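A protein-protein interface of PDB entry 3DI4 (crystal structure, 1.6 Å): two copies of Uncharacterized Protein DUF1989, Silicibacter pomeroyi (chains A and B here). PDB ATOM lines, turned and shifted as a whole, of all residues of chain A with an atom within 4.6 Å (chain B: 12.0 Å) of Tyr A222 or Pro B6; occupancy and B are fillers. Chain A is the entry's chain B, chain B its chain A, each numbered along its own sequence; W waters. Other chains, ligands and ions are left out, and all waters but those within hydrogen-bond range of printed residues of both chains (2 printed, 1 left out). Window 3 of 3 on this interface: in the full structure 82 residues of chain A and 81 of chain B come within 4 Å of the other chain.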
ATOM      1  N   ARG A  70       3.710  15.239 -22.992  1.00  0.00           N
ATOM      2  CA  ARG A  70       4.382  16.086 -22.014  1.00  0.00           C
ATOM      3  C   ARG A  70       3.394  17.134 -21.513  1.00  0.00           C
ATOM      4  O   ARG A  70       2.653  17.724 -22.298  1.00  0.00           O
ATOM      5  CB  ARG A  70       5.613  16.740 -22.657  1.00  0.00           C
ATOM      6  CG  ARG A  70       6.367  17.651 -21.719  1.00  0.00           C
ATOM      7  CD  ARG A  70       7.478  18.423 -22.385  1.00  0.00           C
ATOM      8  NE  ARG A  70       8.546  17.537 -22.785  1.00  0.00           N
ATOM      9  CZ  ARG A  70       9.763  17.952 -23.133  1.00  0.00           C
ATOM     10  NH1 ARG A  70      10.028  19.252 -23.208  1.00  0.00           N
ATOM     11  NH2 ARG A  70      10.700  17.057 -23.412  1.00  0.00           N
ATOM     12  N   ILE A  71       3.391  17.362 -20.201  1.00  0.00           N
ATOM     13  CA  ILE A  71       2.573  18.431 -19.595  1.00  0.00           C
ATOM     14  C   ILE A  71       3.604  19.422 -19.073  1.00  0.00           C
ATOM     15  O   ILE A  71       4.461  19.059 -18.268  1.00  0.00           O
ATOM     16  CB  ILE A  71       1.685  17.954 -18.443  1.00  0.00           C
ATOM     17  CG1 ILE A  71       0.732  16.866 -18.963  1.00  0.00           C
ATOM     18  CG2 ILE A  71       0.941  19.121 -17.836  1.00  0.00           C
ATOM     19  CD1 ILE A  71      -0.035  16.168 -17.848  1.00  0.00           C
ATOM     20  N   SER A  72       3.530  20.653 -19.575  1.00  0.00           N
ATOM     21  CA  SER A  72       4.481  21.706 -19.228  1.00  0.00           C
ATOM     22  C   SER A  72       3.838  22.902 -18.536  1.00  0.00           C
ATOM     23  O   SER A  72       2.705  23.305 -18.851  1.00  0.00           O
ATOM     24  CB  SER A  72       5.191  22.226 -20.493  1.00  0.00           C
ATOM     25  OG  SER A  72       5.965  21.233 -21.117  1.00  0.00           O
ATOM     26  N   GLU A 128      10.249  11.325 -17.674  1.00  0.00           N
ATOM     27  CA  GLU A 128      11.004  12.470 -17.179  1.00  0.00           C
ATOM     28  C   GLU A 128      10.106  13.308 -16.273  1.00  0.00           C
ATOM     29  O   GLU A 128       8.932  13.468 -16.528  1.00  0.00           O
ATOM     30  CB  GLU A 128      11.560  13.295 -18.351  1.00  0.00           C
ATOM     31  CG  GLU A 128      12.270  14.579 -17.963  1.00  0.00           C
ATOM     32  CD  GLU A 128      13.695  14.399 -17.540  1.00  0.00           C
ATOM     33  OE1 GLU A 128      13.926  13.727 -16.513  1.00  0.00           O
ATOM     34  OE2 GLU A 128      14.584  14.975 -18.218  1.00  0.00           O
ATOM     35  N   ASP A 129      10.708  13.807 -15.213  1.00  0.00           N
ATOM     36  CA  ASP A 129      10.057  14.668 -14.244  1.00  0.00           C
ATOM     37  C   ASP A 129      11.061  15.745 -13.860  1.00  0.00           C
ATOM     38  O   ASP A 129      11.990  15.469 -13.099  1.00  0.00           O
ATOM     39  CB  ASP A 129       9.721  13.817 -13.001  1.00  0.00           C
ATOM     40  CG  ASP A 129       9.100  14.604 -11.872  1.00  0.00           C
ATOM     41  OD1 ASP A 129       8.792  15.808 -12.055  1.00  0.00           O
ATOM     42  OD2 ASP A 129       8.914  13.976 -10.776  1.00  0.00           O
ATOM     43  N   THR A 130      10.886  16.967 -14.357  1.00  0.00           N
ATOM     44  CA  THR A 130      11.848  18.029 -14.038  1.00  0.00           C
ATOM     45  C   THR A 130      11.806  18.447 -12.562  1.00  0.00           C
ATOM     46  O   THR A 130      12.736  19.085 -12.069  1.00  0.00           O
ATOM     47  CB  THR A 130      11.657  19.259 -14.925  1.00  0.00           C
ATOM     48  OG1 THR A 130      10.369  19.844 -14.664  1.00  0.00           O
ATOM     49  CG2 THR A 130      11.816  18.873 -16.400  1.00  0.00           C
ATOM     50  N   PHE A 198       2.088  18.433 -10.632  1.00  0.00           N
ATOM     51  CA  PHE A 198       2.772  19.598 -10.074  1.00  0.00           C
ATOM     52  C   PHE A 198       2.318  19.981  -8.681  1.00  0.00           C
ATOM     53  O   PHE A 198       2.955  20.829  -8.075  1.00  0.00           O
ATOM     54  CB  PHE A 198       2.669  20.857 -10.960  1.00  0.00           C
ATOM     55  CG  PHE A 198       3.125  20.667 -12.374  1.00  0.00           C
ATOM     56  CD1 PHE A 198       4.327  20.066 -12.635  1.00  0.00           C
ATOM     57  CD2 PHE A 198       2.402  21.192 -13.429  1.00  0.00           C
ATOM     58  CE1 PHE A 198       4.776  19.904 -13.954  1.00  0.00           C
ATOM     59  CE2 PHE A 198       2.826  21.065 -14.722  1.00  0.00           C
ATOM     60  CZ  PHE A 198       4.002  20.417 -15.004  1.00  0.00           C
ATOM     61  N   GLY A 220       8.479  26.191 -17.617  1.00  0.00           N
ATOM     62  CA  GLY A 220       9.577  25.398 -18.157  1.00  0.00           C
ATOM     63  C   GLY A 220       9.636  23.990 -17.582  1.00  0.00           C
ATOM     64  O   GLY A 220      10.176  23.083 -18.200  1.00  0.00           O
ATOM     65  N   ASP A 221       9.126  23.832 -16.366  1.00  0.00           N
ATOM     66  CA  ASP A 221       9.048  22.514 -15.754  1.00  0.00           C
ATOM     67  C   ASP A 221       8.043  21.680 -16.551  1.00  0.00           C
ATOM     68  O   ASP A 221       7.115  22.187 -17.139  1.00  0.00           O
ATOM     69  CB  ASP A 221       8.618  22.570 -14.288  1.00  0.00           C
ATOM     70  CG  ASP A 221       9.769  22.809 -13.338  1.00  0.00           C
ATOM     71  OD1 ASP A 221      10.807  22.071 -13.379  1.00  0.00           O
ATOM     72  OD2 ASP A 221       9.604  23.741 -12.495  1.00  0.00           O
ATOM     73  N   TYR A 222       8.286  20.379 -16.558  1.00  0.00           N
ATOM     74  CA  TYR A 222       7.401  19.454 -17.223  1.00  0.00           C
ATOM     75  C   TYR A 222       7.447  18.038 -16.609  1.00  0.00           C
ATOM     76  O   TYR A 222       8.380  17.656 -15.899  1.00  0.00           O
ATOM     77  CB  TYR A 222       7.667  19.411 -18.729  1.00  0.00           C
ATOM     78  CG  TYR A 222       9.039  18.954 -19.143  1.00  0.00           C
ATOM     79  CD1 TYR A 222       9.320  17.597 -19.268  1.00  0.00           C
ATOM     80  CD2 TYR A 222      10.059  19.866 -19.402  1.00  0.00           C
ATOM     81  CE1 TYR A 222      10.559  17.162 -19.657  1.00  0.00           C
ATOM     82  CE2 TYR A 222      11.305  19.421 -19.793  1.00  0.00           C
ATOM     83  CZ  TYR A 222      11.553  18.082 -19.930  1.00  0.00           C
ATOM     84  OH  TYR A 222      12.820  17.640 -20.321  1.00  0.00           O
ATOM     85  N   LEU A 223       6.381  17.299 -16.918  1.00  0.00           N
ATOM     86  CA  LEU A 223       6.248  15.887 -16.584  1.00  0.00           C
ATOM     87  C   LEU A 223       5.929  15.189 -17.901  1.00  0.00           C
ATOM     88  O   LEU A 223       4.948  15.525 -18.579  1.00  0.00           O
ATOM     89  CB  LEU A 223       5.151  15.656 -15.511  1.00  0.00           C
ATOM     90  CG  LEU A 223       5.040  14.252 -14.941  1.00  0.00           C
ATOM     91  CD1 LEU A 223       6.310  13.843 -14.165  1.00  0.00           C
ATOM     92  CD2 LEU A 223       3.819  14.193 -14.013  1.00  0.00           C
ATOM     93  N   GLU A 224       6.738  14.184 -18.245  1.00  0.00           N
ATOM     94  CA  GLU A 224       6.606  13.519 -19.542  1.00  0.00           C
ATOM     95  C   GLU A 224       6.385  12.023 -19.385  1.00  0.00           C
ATOM     96  O   GLU A 224       7.046  11.391 -18.544  1.00  0.00           O
ATOM     97  CB  GLU A 224       7.834  13.832 -20.405  1.00  0.00           C
ATOM     98  CG  GLU A 224       7.677  13.377 -21.828  1.00  0.00           C
ATOM     99  CD  GLU A 224       8.819  13.877 -22.671  1.00  0.00           C
ATOM    100  OE1 GLU A 224       9.929  13.333 -22.544  1.00  0.00           O
ATOM    101  OE2 GLU A 224       8.601  14.781 -23.470  1.00  0.00           O
ATOM    102  N   MET B   2      30.260  22.079 -15.164  1.00  0.00           N
ATOM    103  CA  MET B   2      29.372  20.935 -15.323  1.00  0.00           C
ATOM    104  C   MET B   2      28.025  21.436 -15.827  1.00  0.00           C
ATOM    105  O   MET B   2      27.537  22.465 -15.357  1.00  0.00           O
ATOM    106  CB  MET B   2      29.172  20.265 -13.967  1.00  0.00           C
ATOM    107  CG  MET B   2      30.467  19.838 -13.267  1.00  0.00           C
ATOM    108  SD  MET B   2      30.862  17.976 -13.589  1.00  0.00           S
ATOM    109  CE  MET B   2      31.270  18.042 -15.463  1.00  0.00           C
ATOM    110  N   THR B   3      27.411  20.700 -16.754  1.00  0.00           N
ATOM    111  CA  THR B   3      26.127  21.142 -17.307  1.00  0.00           C
ATOM    112  C   THR B   3      24.956  20.595 -16.473  1.00  0.00           C
ATOM    113  O   THR B   3      25.071  19.587 -15.777  1.00  0.00           O
ATOM    114  CB  THR B   3      26.000  20.809 -18.823  1.00  0.00           C
ATOM    115  OG1 THR B   3      24.743  21.286 -19.331  1.00  0.00           O
ATOM    116  CG2 THR B   3      26.121  19.331 -19.057  1.00  0.00           C
ATOM    117  N   ASP B   4      23.840  21.315 -16.513  1.00  0.00           N
ATOM    118  CA  ASP B   4      22.647  20.927 -15.755  1.00  0.00           C
ATOM    119  C   ASP B   4      21.718  20.061 -16.602  1.00  0.00           C
ATOM    120  O   ASP B   4      21.706  20.186 -17.840  1.00  0.00           O
ATOM    121  CB  ASP B   4      21.902  22.176 -15.275  1.00  0.00           C
ATOM    122  CG  ASP B   4      22.790  23.089 -14.455  1.00  0.00           C
ATOM    123  OD1 ASP B   4      23.382  22.608 -13.455  1.00  0.00           O
ATOM    124  OD2 ASP B   4      22.919  24.274 -14.828  1.00  0.00           O
ATOM    125  N   ALA B   5      20.977  19.164 -15.940  1.00  0.00           N
ATOM    126  CA  ALA B   5      19.979  18.329 -16.588  1.00  0.00           C
ATOM    127  C   ALA B   5      18.618  18.885 -16.198  1.00  0.00           C
ATOM    128  O   ALA B   5      18.511  19.619 -15.190  1.00  0.00           O
ATOM    129  CB  ALA B   5      20.107  16.879 -16.133  1.00  0.00           C
ATOM    130  N   PRO B   6      17.584  18.574 -16.999  1.00  0.00           N
ATOM    131  CA  PRO B   6      16.232  19.037 -16.697  1.00  0.00           C
ATOM    132  C   PRO B   6      15.736  18.814 -15.264  1.00  0.00           C
ATOM    133  O   PRO B   6      15.037  19.704 -14.741  1.00  0.00           O
ATOM    134  CB  PRO B   6      15.373  18.233 -17.676  1.00  0.00           C
ATOM    135  CG  PRO B   6      16.239  18.124 -18.889  1.00  0.00           C
ATOM    136  CD  PRO B   6      17.613  17.849 -18.290  1.00  0.00           C
ATOM    137  N   ALA B   7      16.076  17.669 -14.670  1.00  0.00           N
ATOM    138  CA  ALA B   7      15.537  17.287 -13.341  1.00  0.00           C
ATOM    139  C   ALA B   7      16.437  17.658 -12.156  1.00  0.00           C
ATOM    140  O   ALA B   7      16.119  17.320 -11.010  1.00  0.00           O
ATOM    141  CB  ALA B   7      15.223  15.798 -13.313  1.00  0.00           C
ATOM    142  N   ASP B   8      17.538  18.360 -12.402  1.00  0.00           N
ATOM    143  CA  ASP B   8      18.455  18.719 -11.314  1.00  0.00           C
ATOM    144  C   ASP B   8      17.876  19.812 -10.392  1.00  0.00           C
ATOM    145  O   ASP B   8      17.098  20.686 -10.809  1.00  0.00           O
ATOM    146  CB  ASP B   8      19.790  19.241 -11.849  1.00  0.00           C
ATOM    147  CG  ASP B   8      20.577  18.208 -12.600  1.00  0.00           C
ATOM    148  OD1 ASP B   8      20.243  17.001 -12.589  1.00  0.00           O
ATOM    149  OD2 ASP B   8      21.555  18.653 -13.215  1.00  0.00           O
ATOM    150  N   ALA B   9      18.259  19.767  -9.125  1.00  0.00           N
ATOM    151  CA  ALA B   9      17.742  20.707  -8.132  1.00  0.00           C
ATOM    152  C   ALA B   9      18.153  22.139  -8.464  1.00  0.00           C
ATOM    153  O   ALA B   9      19.309  22.385  -8.860  1.00  0.00           O
ATOM    154  CB  ALA B   9      18.235  20.320  -6.718  1.00  0.00           C
ATOM    155  N   PRO B  10      17.214  23.091  -8.343  1.00  0.00           N
ATOM    156  CA  PRO B  10      17.529  24.530  -8.435  1.00  0.00           C
ATOM    157  C   PRO B  10      18.215  25.073  -7.183  1.00  0.00           C
ATOM    158  O   PRO B  10      18.216  24.433  -6.142  1.00  0.00           O
ATOM    159  CB  PRO B  10      16.164  25.195  -8.593  1.00  0.00           C
ATOM    160  CG  PRO B  10      15.199  24.235  -7.909  1.00  0.00           C
ATOM    161  CD  PRO B  10      15.783  22.864  -8.025  1.00  0.00           C
ATOM    162  N   LEU B  11      18.813  26.263  -7.282  1.00  0.00           N
ATOM    163  CA  LEU B  11      19.548  26.777  -6.155  1.00  0.00           C
ATOM    164  C   LEU B  11      18.663  27.019  -4.931  1.00  0.00           C
ATOM    165  O   LEU B  11      19.141  26.937  -3.816  1.00  0.00           O
ATOM    166  CB  LEU B  11      20.300  28.063  -6.533  1.00  0.00           C
ATOM    167  CG  LEU B  11      19.484  29.348  -6.515  1.00  0.00           C
ATOM    168  CD1 LEU B  11      20.454  30.572  -6.585  1.00  0.00           C
ATOM    169  CD2 LEU B  11      18.467  29.358  -7.638  1.00  0.00           C
ATOM    170  N   ASP B  12      17.391  27.318  -5.162  1.00  0.00           N
ATOM    171  CA  ASP B  12      16.441  27.588  -4.085  1.00  0.00           C
ATOM    172  C   ASP B  12      15.601  26.349  -3.740  1.00  0.00           C
ATOM    173  O   ASP B  12      14.514  26.500  -3.190  1.00  0.00           O
ATOM    174  CB  ASP B  12      15.523  28.769  -4.412  1.00  0.00           C
ATOM    175  CG  ASP B  12      14.665  28.536  -5.632  1.00  0.00           C
ATOM    176  OD1 ASP B  12      15.142  27.891  -6.585  1.00  0.00           O
ATOM    177  OD2 ASP B  12      13.516  29.045  -5.718  1.00  0.00           O
ATOM    178  N   ALA B  13      16.112  25.141  -4.013  1.00  0.00           N
ATOM    179  CA  ALA B  13      15.401  23.903  -3.615  1.00  0.00           C
ATOM    180  C   ALA B  13      14.947  23.914  -2.146  1.00  0.00           C
ATOM    181  O   ALA B  13      13.802  23.605  -1.833  1.00  0.00           O
ATOM    182  CB  ALA B  13      16.286  22.654  -3.870  1.00  0.00           C
ATOM    183  N   ARG B  16      11.993  26.187  -1.372  1.00  0.00           N
ATOM    184  CA  ARG B  16      10.717  25.664  -1.887  1.00  0.00           C
ATOM    185  C   ARG B  16      10.226  24.558  -0.973  1.00  0.00           C
ATOM    186  O   ARG B  16       9.015  24.439  -0.750  1.00  0.00           O
ATOM    187  CB  ARG B  16      10.849  25.183  -3.346  1.00  0.00           C
ATOM    188  CG  ARG B  16      11.299  26.271  -4.304  1.00  0.00           C
ATOM    189  CD  ARG B  16      11.188  25.844  -5.725  1.00  0.00           C
ATOM    190  NE  ARG B  16      12.074  26.588  -6.609  1.00  0.00           N
ATOM    191  CZ  ARG B  16      12.201  26.346  -7.904  1.00  0.00           C
ATOM    192  NH1 ARG B  16      11.434  25.441  -8.525  1.00  0.00           N
ATOM    193  NH2 ARG B  16      13.101  27.047  -8.591  1.00  0.00           N
ATOM    194  N   ARG B  17      11.148  23.745  -0.468  1.00  0.00           N
ATOM    195  CA  ARG B  17      10.812  22.692   0.477  1.00  0.00           C
ATOM    196  C   ARG B  17      10.331  23.241   1.831  1.00  0.00           C
ATOM    197  O   ARG B  17       9.549  22.595   2.521  1.00  0.00           O
ATOM    198  CB  ARG B  17      11.998  21.749   0.679  1.00  0.00           C
ATOM    199  CG  ARG B  17      12.311  20.892  -0.533  1.00  0.00           C
ATOM    200  CD  ARG B  17      13.277  19.807  -0.166  1.00  0.00           C
ATOM    201  NE  ARG B  17      13.743  19.050  -1.316  1.00  0.00           N
ATOM    202  CZ  ARG B  17      14.966  19.140  -1.863  1.00  0.00           C
ATOM    203  NH1 ARG B  17      15.902  19.943  -1.396  1.00  0.00           N
ATOM    204  NH2 ARG B  17      15.250  18.358  -2.900  1.00  0.00           N
HETATM  205  O   HOH W   1      17.007  15.439 -16.087  1.00  0.00           O
HETATM  206  O   HOH W   2      11.882  24.697 -11.268  1.00  0.00           O
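Glu A128 touches Pro B6 (OE2 to CB, 3.4 Å). Ala B7 touches Asp A129 (CB to O, 3.3 Å). Pro B6 touches Thr A130. Ala B7 touches Thr A130. Tyr A222 touches Pro B6.
Arg A70 touches none of the printed residues of chain B. No residue of chain B comes within 4 Å of Ser A72. Printed residues of chain B within 4 Å of Glu A128: Pro B6. Of chain B, only Ala B7 (3.3 Å) comes within 4 Å of Asp A129. Of chain B, only Pro B6 (3.4 Å) and Ala B7 (3.6 Å) come within 4 Å of Thr A130. No residue of chain B comes within 4 Å of Gly A220. Asp A221 touches none of the printed residues of chain B. Tyr A222 touches one residue of chain B. No residue of chain B comes within 4 Å of Glu A224. Printed residues of chain A within 4 Å of Ala B7: Asp A129 and Thr A130. Asp B12 touches none of the printed residues of chain A. The nearest residue of chain B that does not touch Tyr A222 is Ala B7 (6.5 Å). The nearest printed residue of chain A that does not touch Ala B7 is Glu A128 (4.03 Å).
No position is printed for both chains.
Of the 14 printed residues of chain B, 2 touch a printed residue of chain A. Hydrophobic or aromatic side chains of chain B that line the printed part of chain A: Pro B6 and Ala B7. Hydrophobic or aromatic side chains of chain A that line the printed part of chain B: Tyr A222. Among the printed residues, 5 pairs touch across the chains.
The backbone carbonyl oxygen (O) of Glu A128 sits at hydrogen-bond distance from the backbone NH (N) of Glu A224. The side-chain carboxylate (OD1) of Asp A221 is in hydrogen-bond range of the side-chain hydroxyl (OG1) of Thr A130 (2.6 Å). OG1 of Thr A130 is in hydrogen-bond range of N of Tyr A222.
Water W2 lies within hydrogen-bond range of the side-chain carboxylate (OD2) of Asp A221 and the guanidinium group (NH1) of Arg B16. Water W1 lies within hydrogen-bond range of the backbone NH of Ala B7 (2.8 Å) and the side-chain carboxylate of Glu A128 (3.3 Å).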
